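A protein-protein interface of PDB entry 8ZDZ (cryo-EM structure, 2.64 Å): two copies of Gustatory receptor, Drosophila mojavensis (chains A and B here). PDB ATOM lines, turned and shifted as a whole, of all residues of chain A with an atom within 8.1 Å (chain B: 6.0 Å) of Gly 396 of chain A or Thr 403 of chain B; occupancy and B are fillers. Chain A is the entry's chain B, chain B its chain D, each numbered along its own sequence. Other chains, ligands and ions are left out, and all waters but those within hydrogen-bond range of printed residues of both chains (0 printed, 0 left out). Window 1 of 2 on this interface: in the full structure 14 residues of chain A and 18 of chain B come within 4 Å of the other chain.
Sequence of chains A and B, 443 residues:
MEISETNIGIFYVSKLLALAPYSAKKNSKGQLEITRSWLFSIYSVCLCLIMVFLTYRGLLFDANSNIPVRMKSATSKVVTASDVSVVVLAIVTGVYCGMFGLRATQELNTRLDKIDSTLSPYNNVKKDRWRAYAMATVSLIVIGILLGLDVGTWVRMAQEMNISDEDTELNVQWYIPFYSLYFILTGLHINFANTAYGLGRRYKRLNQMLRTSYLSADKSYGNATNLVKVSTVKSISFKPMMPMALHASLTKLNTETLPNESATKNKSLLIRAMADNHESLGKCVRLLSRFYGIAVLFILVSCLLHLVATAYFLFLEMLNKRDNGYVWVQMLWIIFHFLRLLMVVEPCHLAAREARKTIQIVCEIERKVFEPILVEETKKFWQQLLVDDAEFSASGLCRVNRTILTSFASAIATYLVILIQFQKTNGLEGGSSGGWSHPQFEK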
ATOM      1  N   SER A 289     -12.519 -10.312  -5.936  1.00  0.00           N
ATOM      2  CA  SER A 289     -13.434 -10.916  -6.896  1.00  0.00           C
ATOM      3  C   SER A 289     -14.112  -9.849  -7.746  1.00  0.00           C
ATOM      4  O   SER A 289     -14.139  -9.944  -8.974  1.00  0.00           O
ATOM      5  CB  SER A 289     -14.470 -11.769  -6.168  1.00  0.00           C
ATOM      6  OG  SER A 289     -14.949 -12.808  -7.002  1.00  0.00           O
ATOM      7  N   GLY A 293     -12.934 -10.353 -11.518  1.00  0.00           N
ATOM      8  CA  GLY A 293     -13.721 -11.509 -11.896  1.00  0.00           C
ATOM      9  C   GLY A 293     -13.767 -11.803 -13.378  1.00  0.00           C
ATOM     10  O   GLY A 293     -13.429 -12.909 -13.808  1.00  0.00           O
ATOM     11  N   ILE A 294     -14.191 -10.819 -14.170  1.00  0.00           N
ATOM     12  CA  ILE A 294     -14.295 -11.039 -15.607  1.00  0.00           C
ATOM     13  C   ILE A 294     -12.913 -11.224 -16.223  1.00  0.00           C
ATOM     14  O   ILE A 294     -12.741 -12.021 -17.156  1.00  0.00           O
ATOM     15  CB  ILE A 294     -15.085  -9.886 -16.253  1.00  0.00           C
ATOM     16  CG1 ILE A 294     -15.295 -10.143 -17.743  1.00  0.00           C
ATOM     17  CG2 ILE A 294     -14.419  -8.547 -15.986  1.00  0.00           C
ATOM     18  CD1 ILE A 294     -16.390 -11.141 -18.029  1.00  0.00           C
ATOM     19  N   LEU A 297     -11.949 -14.760 -15.499  1.00  0.00           N
ATOM     20  CA  LEU A 297     -12.746 -15.650 -16.334  1.00  0.00           C
ATOM     21  C   LEU A 297     -12.180 -15.725 -17.746  1.00  0.00           C
ATOM     22  O   LEU A 297     -12.020 -16.816 -18.314  1.00  0.00           O
ATOM     23  CB  LEU A 297     -14.197 -15.175 -16.357  1.00  0.00           C
ATOM     24  CG  LEU A 297     -15.089 -15.765 -17.446  1.00  0.00           C
ATOM     25  CD1 LEU A 297     -15.392 -17.220 -17.146  1.00  0.00           C
ATOM     26  CD2 LEU A 297     -16.368 -14.961 -17.569  1.00  0.00           C
ATOM     27  N   PHE A 392     -12.857 -17.517  -4.299  1.00  0.00           N
ATOM     28  CA  PHE A 392     -12.818 -16.534  -5.369  1.00  0.00           C
ATOM     29  C   PHE A 392     -13.756 -16.965  -6.487  1.00  0.00           C
ATOM     30  O   PHE A 392     -13.697 -18.105  -6.955  1.00  0.00           O
ATOM     31  CB  PHE A 392     -11.392 -16.384  -5.889  1.00  0.00           C
ATOM     32  CG  PHE A 392     -11.247 -15.378  -6.990  1.00  0.00           C
ATOM     33  CD1 PHE A 392     -11.366 -15.756  -8.315  1.00  0.00           C
ATOM     34  CD2 PHE A 392     -10.976 -14.056  -6.702  1.00  0.00           C
ATOM     35  CE1 PHE A 392     -11.229 -14.835  -9.327  1.00  0.00           C
ATOM     36  CE2 PHE A 392     -10.836 -13.132  -7.711  1.00  0.00           C
ATOM     37  CZ  PHE A 392     -10.963 -13.521  -9.024  1.00  0.00           C
ATOM     38  N   SER A 393     -14.623 -16.056  -6.915  1.00  0.00           N
ATOM     39  CA  SER A 393     -15.597 -16.332  -7.960  1.00  0.00           C
ATOM     40  C   SER A 393     -15.276 -15.493  -9.188  1.00  0.00           C
ATOM     41  O   SER A 393     -15.103 -14.275  -9.084  1.00  0.00           O
ATOM     42  CB  SER A 393     -17.016 -16.039  -7.477  1.00  0.00           C
ATOM     43  OG  SER A 393     -17.173 -14.662  -7.188  1.00  0.00           O
ATOM     44  N   ALA A 394     -15.200 -16.146 -10.348  1.00  0.00           N
ATOM     45  CA  ALA A 394     -14.925 -15.463 -11.610  1.00  0.00           C
ATOM     46  C   ALA A 394     -16.192 -14.748 -12.078  1.00  0.00           C
ATOM     47  O   ALA A 394     -16.856 -15.140 -13.041  1.00  0.00           O
ATOM     48  CB  ALA A 394     -14.416 -16.449 -12.651  1.00  0.00           C
ATOM     49  N   SER A 395     -16.521 -13.675 -11.362  1.00  0.00           N
ATOM     50  CA  SER A 395     -17.719 -12.874 -11.617  1.00  0.00           C
ATOM     51  C   SER A 395     -18.988 -13.717 -11.554  1.00  0.00           C
ATOM     52  O   SER A 395     -19.962 -13.445 -12.256  1.00  0.00           O
ATOM     53  CB  SER A 395     -17.629 -12.144 -12.961  1.00  0.00           C
ATOM     54  OG  SER A 395     -17.808 -13.040 -14.039  1.00  0.00           O
ATOM     55  N   GLY A 396     -18.983 -14.751 -10.713  1.00  0.00           N
ATOM     56  CA  GLY A 396     -20.151 -15.571 -10.488  1.00  0.00           C
ATOM     57  C   GLY A 396     -20.305 -16.757 -11.414  1.00  0.00           C
ATOM     58  O   GLY A 396     -21.104 -17.653 -11.114  1.00  0.00           O
ATOM     59  N   LEU A 397     -19.570 -16.800 -12.526  1.00  0.00           N
ATOM     60  CA  LEU A 397     -19.732 -17.907 -13.464  1.00  0.00           C
ATOM     61  C   LEU A 397     -19.171 -19.205 -12.902  1.00  0.00           C
ATOM     62  O   LEU A 397     -19.739 -20.278 -13.126  1.00  0.00           O
ATOM     63  CB  LEU A 397     -19.074 -17.570 -14.800  1.00  0.00           C
ATOM     64  CG  LEU A 397     -19.925 -16.746 -15.763  1.00  0.00           C
ATOM     65  CD1 LEU A 397     -19.667 -15.266 -15.583  1.00  0.00           C
ATOM     66  CD2 LEU A 397     -19.658 -17.168 -17.194  1.00  0.00           C
ATOM     67  N   CYS A 398     -18.056 -19.136 -12.181  1.00  0.00           N
ATOM     68  CA  CYS A 398     -17.447 -20.342 -11.641  1.00  0.00           C
ATOM     69  C   CYS A 398     -16.634 -19.984 -10.409  1.00  0.00           C
ATOM     70  O   CYS A 398     -16.258 -18.829 -10.202  1.00  0.00           O
ATOM     71  CB  CYS A 398     -16.567 -21.039 -12.680  1.00  0.00           C
ATOM     72  SG  CYS A 398     -15.061 -20.139 -13.096  1.00  0.00           S
ATOM     73  N   ARG A 399     -16.370 -21.000  -9.594  1.00  0.00           N
ATOM     74  CA  ARG A 399     -15.513 -20.874  -8.425  1.00  0.00           C
ATOM     75  C   ARG A 399     -14.105 -21.304  -8.804  1.00  0.00           C
ATOM     76  O   ARG A 399     -13.913 -22.386  -9.368  1.00  0.00           O
ATOM     77  CB  ARG A 399     -16.035 -21.728  -7.269  1.00  0.00           C
ATOM     78  CG  ARG A 399     -16.492 -20.932  -6.066  1.00  0.00           C
ATOM     79  CD  ARG A 399     -17.900 -20.403  -6.260  1.00  0.00           C
ATOM     80  NE  ARG A 399     -18.168 -19.250  -5.411  1.00  0.00           N
ATOM     81  CZ  ARG A 399     -18.643 -19.324  -4.175  1.00  0.00           C
ATOM     82  NH1 ARG A 399     -18.922 -20.488  -3.611  1.00  0.00           N
ATOM     83  NH2 ARG A 399     -18.846 -18.204  -3.489  1.00  0.00           N
ATOM     84  N   VAL B 345     -31.054 -15.071 -17.114  1.00  0.00           N
ATOM     85  CA  VAL B 345     -30.150 -15.572 -16.083  1.00  0.00           C
ATOM     86  C   VAL B 345     -29.805 -14.488 -15.068  1.00  0.00           C
ATOM     87  O   VAL B 345     -29.871 -14.713 -13.855  1.00  0.00           O
ATOM     88  CB  VAL B 345     -28.884 -16.156 -16.737  1.00  0.00           C
ATOM     89  CG1 VAL B 345     -27.710 -16.085 -15.785  1.00  0.00           C
ATOM     90  CG2 VAL B 345     -29.127 -17.584 -17.176  1.00  0.00           C
ATOM     91  N   HIS B 349     -29.732 -14.606 -10.775  1.00  0.00           N
ATOM     92  CA  HIS B 349     -28.454 -14.613 -10.071  1.00  0.00           C
ATOM     93  C   HIS B 349     -28.321 -13.402  -9.164  1.00  0.00           C
ATOM     94  O   HIS B 349     -27.818 -13.510  -8.041  1.00  0.00           O
ATOM     95  CB  HIS B 349     -27.302 -14.657 -11.070  1.00  0.00           C
ATOM     96  CG  HIS B 349     -25.953 -14.541 -10.434  1.00  0.00           C
ATOM     97  ND1 HIS B 349     -25.165 -13.419 -10.559  1.00  0.00           N
ATOM     98  CD2 HIS B 349     -25.253 -15.409  -9.667  1.00  0.00           C
ATOM     99  CE1 HIS B 349     -24.038 -13.597  -9.894  1.00  0.00           C
ATOM    100  NE2 HIS B 349     -24.066 -14.797  -9.345  1.00  0.00           N
ATOM    101  N   ASN B 401     -28.764 -19.412 -12.421  1.00  0.00           N
ATOM    102  CA  ASN B 401     -27.826 -18.370 -12.032  1.00  0.00           C
ATOM    103  C   ASN B 401     -26.793 -18.240 -13.143  1.00  0.00           C
ATOM    104  O   ASN B 401     -26.927 -18.850 -14.208  1.00  0.00           O
ATOM    105  CB  ASN B 401     -27.189 -18.677 -10.672  1.00  0.00           C
ATOM    106  CG  ASN B 401     -26.747 -20.116 -10.545  1.00  0.00           C
ATOM    107  OD1 ASN B 401     -26.470 -20.782 -11.540  1.00  0.00           O
ATOM    108  ND2 ASN B 401     -26.674 -20.605  -9.315  1.00  0.00           N
ATOM    109  N   ARG B 402     -25.753 -17.443 -12.897  1.00  0.00           N
ATOM    110  CA  ARG B 402     -24.743 -17.221 -13.924  1.00  0.00           C
ATOM    111  C   ARG B 402     -23.977 -18.493 -14.258  1.00  0.00           C
ATOM    112  O   ARG B 402     -23.450 -18.612 -15.369  1.00  0.00           O
ATOM    113  CB  ARG B 402     -23.781 -16.120 -13.485  1.00  0.00           C
ATOM    114  CG  ARG B 402     -24.031 -14.793 -14.176  1.00  0.00           C
ATOM    115  CD  ARG B 402     -22.911 -13.807 -13.919  1.00  0.00           C
ATOM    116  NE  ARG B 402     -23.247 -12.867 -12.859  1.00  0.00           N
ATOM    117  CZ  ARG B 402     -22.911 -11.585 -12.865  1.00  0.00           C
ATOM    118  NH1 ARG B 402     -22.229 -11.054 -13.866  1.00  0.00           N
ATOM    119  NH2 ARG B 402     -23.270 -10.815 -11.842  1.00  0.00           N
ATOM    120  N   THR B 403     -23.922 -19.452 -13.330  1.00  0.00           N
ATOM    121  CA  THR B 403     -23.254 -20.719 -13.605  1.00  0.00           C
ATOM    122  C   THR B 403     -23.830 -21.396 -14.840  1.00  0.00           C
ATOM    123  O   THR B 403     -23.095 -22.057 -15.585  1.00  0.00           O
ATOM    124  CB  THR B 403     -23.368 -21.647 -12.397  1.00  0.00           C
ATOM    125  OG1 THR B 403     -22.907 -20.965 -11.225  1.00  0.00           O
ATOM    126  CG2 THR B 403     -22.533 -22.896 -12.601  1.00  0.00           C
ATOM    127  N   ILE B 404     -25.130 -21.211 -15.090  1.00  0.00           N
ATOM    128  CA  ILE B 404     -25.764 -21.781 -16.275  1.00  0.00           C
ATOM    129  C   ILE B 404     -24.988 -21.393 -17.524  1.00  0.00           C
ATOM    130  O   ILE B 404     -24.723 -22.232 -18.394  1.00  0.00           O
ATOM    131  CB  ILE B 404     -27.234 -21.329 -16.363  1.00  0.00           C
ATOM    132  CG1 ILE B 404     -28.074 -22.026 -15.290  1.00  0.00           C
ATOM    133  CG2 ILE B 404     -27.788 -21.567 -17.757  1.00  0.00           C
ATOM    134  CD1 ILE B 404     -28.841 -23.226 -15.791  1.00  0.00           C
ATOM    135  N   LEU B 405     -24.577 -20.124 -17.609  1.00  0.00           N
ATOM    136  CA  LEU B 405     -23.802 -19.662 -18.755  1.00  0.00           C
ATOM    137  C   LEU B 405     -22.614 -20.578 -19.006  1.00  0.00           C
ATOM    138  O   LEU B 405     -22.424 -21.076 -20.122  1.00  0.00           O
ATOM    139  CB  LEU B 405     -23.330 -18.227 -18.526  1.00  0.00           C
ATOM    140  CG  LEU B 405     -24.397 -17.160 -18.305  1.00  0.00           C
ATOM    141  CD1 LEU B 405     -23.754 -15.797 -18.147  1.00  0.00           C
ATOM    142  CD2 LEU B 405     -25.378 -17.150 -19.452  1.00  0.00           C
ATOM    143  N   THR B 406     -21.833 -20.852 -17.957  1.00  0.00           N
ATOM    144  CA  THR B 406     -20.690 -21.744 -18.096  1.00  0.00           C
ATOM    145  C   THR B 406     -21.116 -23.070 -18.705  1.00  0.00           C
ATOM    146  O   THR B 406     -20.549 -23.520 -19.709  1.00  0.00           O
ATOM    147  CB  THR B 406     -20.028 -21.970 -16.738  1.00  0.00           C
ATOM    148  OG1 THR B 406     -19.408 -20.758 -16.297  1.00  0.00           O
ATOM    149  CG2 THR B 406     -18.979 -23.060 -16.837  1.00  0.00           C
ATOM    150  N   SER B 407     -22.162 -23.680 -18.141  1.00  0.00           N
ATOM    151  CA  SER B 407     -22.652 -24.948 -18.666  1.00  0.00           C
ATOM    152  C   SER B 407     -22.974 -24.823 -20.146  1.00  0.00           C
ATOM    153  O   SER B 407     -22.560 -25.661 -20.957  1.00  0.00           O
ATOM    154  CB  SER B 407     -23.883 -25.400 -17.883  1.00  0.00           C
ATOM    155  OG  SER B 407     -23.610 -25.451 -16.496  1.00  0.00           O
ATOM    156  N   PHE B 408     -23.662 -23.742 -20.522  1.00  0.00           N
ATOM    157  CA  PHE B 408     -24.005 -23.548 -21.925  1.00  0.00           C
ATOM    158  C   PHE B 408     -22.753 -23.530 -22.784  1.00  0.00           C
ATOM    159  O   PHE B 408     -22.696 -24.198 -23.823  1.00  0.00           O
ATOM    160  CB  PHE B 408     -24.802 -22.259 -22.100  1.00  0.00           C
ATOM    161  CG  PHE B 408     -26.283 -22.441 -21.956  1.00  0.00           C
ATOM    162  CD1 PHE B 408     -26.796 -23.402 -21.105  1.00  0.00           C
ATOM    163  CD2 PHE B 408     -27.163 -21.652 -22.673  1.00  0.00           C
ATOM    164  CE1 PHE B 408     -28.156 -23.571 -20.969  1.00  0.00           C
ATOM    165  CE2 PHE B 408     -28.524 -21.817 -22.541  1.00  0.00           C
ATOM    166  CZ  PHE B 408     -29.020 -22.778 -21.688  1.00  0.00           C
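Of the 12 printed residues of chain A, 3 touch a printed residue of chain B.
Hydrophobic or aromatic side chains of chain A that line the printed part of chain B: Leu 397.
Of the 10 printed residues of chain B, 3 touch a printed residue of chain A.
Printed residues of chain B that touch a printed residue of chain A: Arg 402, Thr 403 and Thr 406.
Among the printed residues, 6 pairs touch across the chains.
Among the printed residues, no Asp or Glu carboxylate lies within 4 Å of a Lys or Arg side-chain nitrogen of the other chain.
Gly 396 of chain A touches just these residues of chain B: Arg 402 and Thr 403.
Thr 403 of chain B touches just these residues of chain A: Gly 396 and Leu 397.
Of the printed residues of chain B, Leu 397 of chain A touches Arg 402 (3.9 Å), Thr 403 (3.6 Å) and Thr 406 (3.2 Å).
Of the printed residues of chain B, Ser 395 of chain A touches Arg 402.
Printed residues of chain A within 4 Å of Arg 402 of chain B: Ser 395 (3.4 Å), Gly 396 (3.9 Å) and Leu 397 (3.9 Å).
Asn 401 of chain B touches none of the printed residues of chain A.
The nearest printed residue of chain A that does not touch Arg 402 of chain B is Ala 394 of chain A (6.3 Å).
OD1 of Asn 401 of chain B lies close to N of Thr 403 of chain B (3.4 Å).
A ring nitrogen (ND1) of His 349 of chain B sits at hydrogen-bond distance from the guanidinium group (NE) of Arg 402 of chain B, at 3.0 Å.
The side-chain hydroxyl (OG1) of Thr 406 of chain B is in hydrogen-bond range of the backbone carbonyl oxygen (O) of Leu 397 of chain A, at 3.2 Å.
The backbone carbonyl oxygen (O) of Ser 395 of chain A lies within hydrogen-bond range of the guanidinium group (NE) of Arg 402 of chain B (3.4 Å).
No position is printed for both chains.
O of Gly 396 of chain A touches CB of Arg 402 of chain B, at 3.9 Å.
Thr 403 of chain B touches Gly 396 of chain A.
Leu 397 of chain A touches Arg 402 of chain B.
Thr 403 of chain B touches Leu 397 of chain A (CA to O, 3.6 Å).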
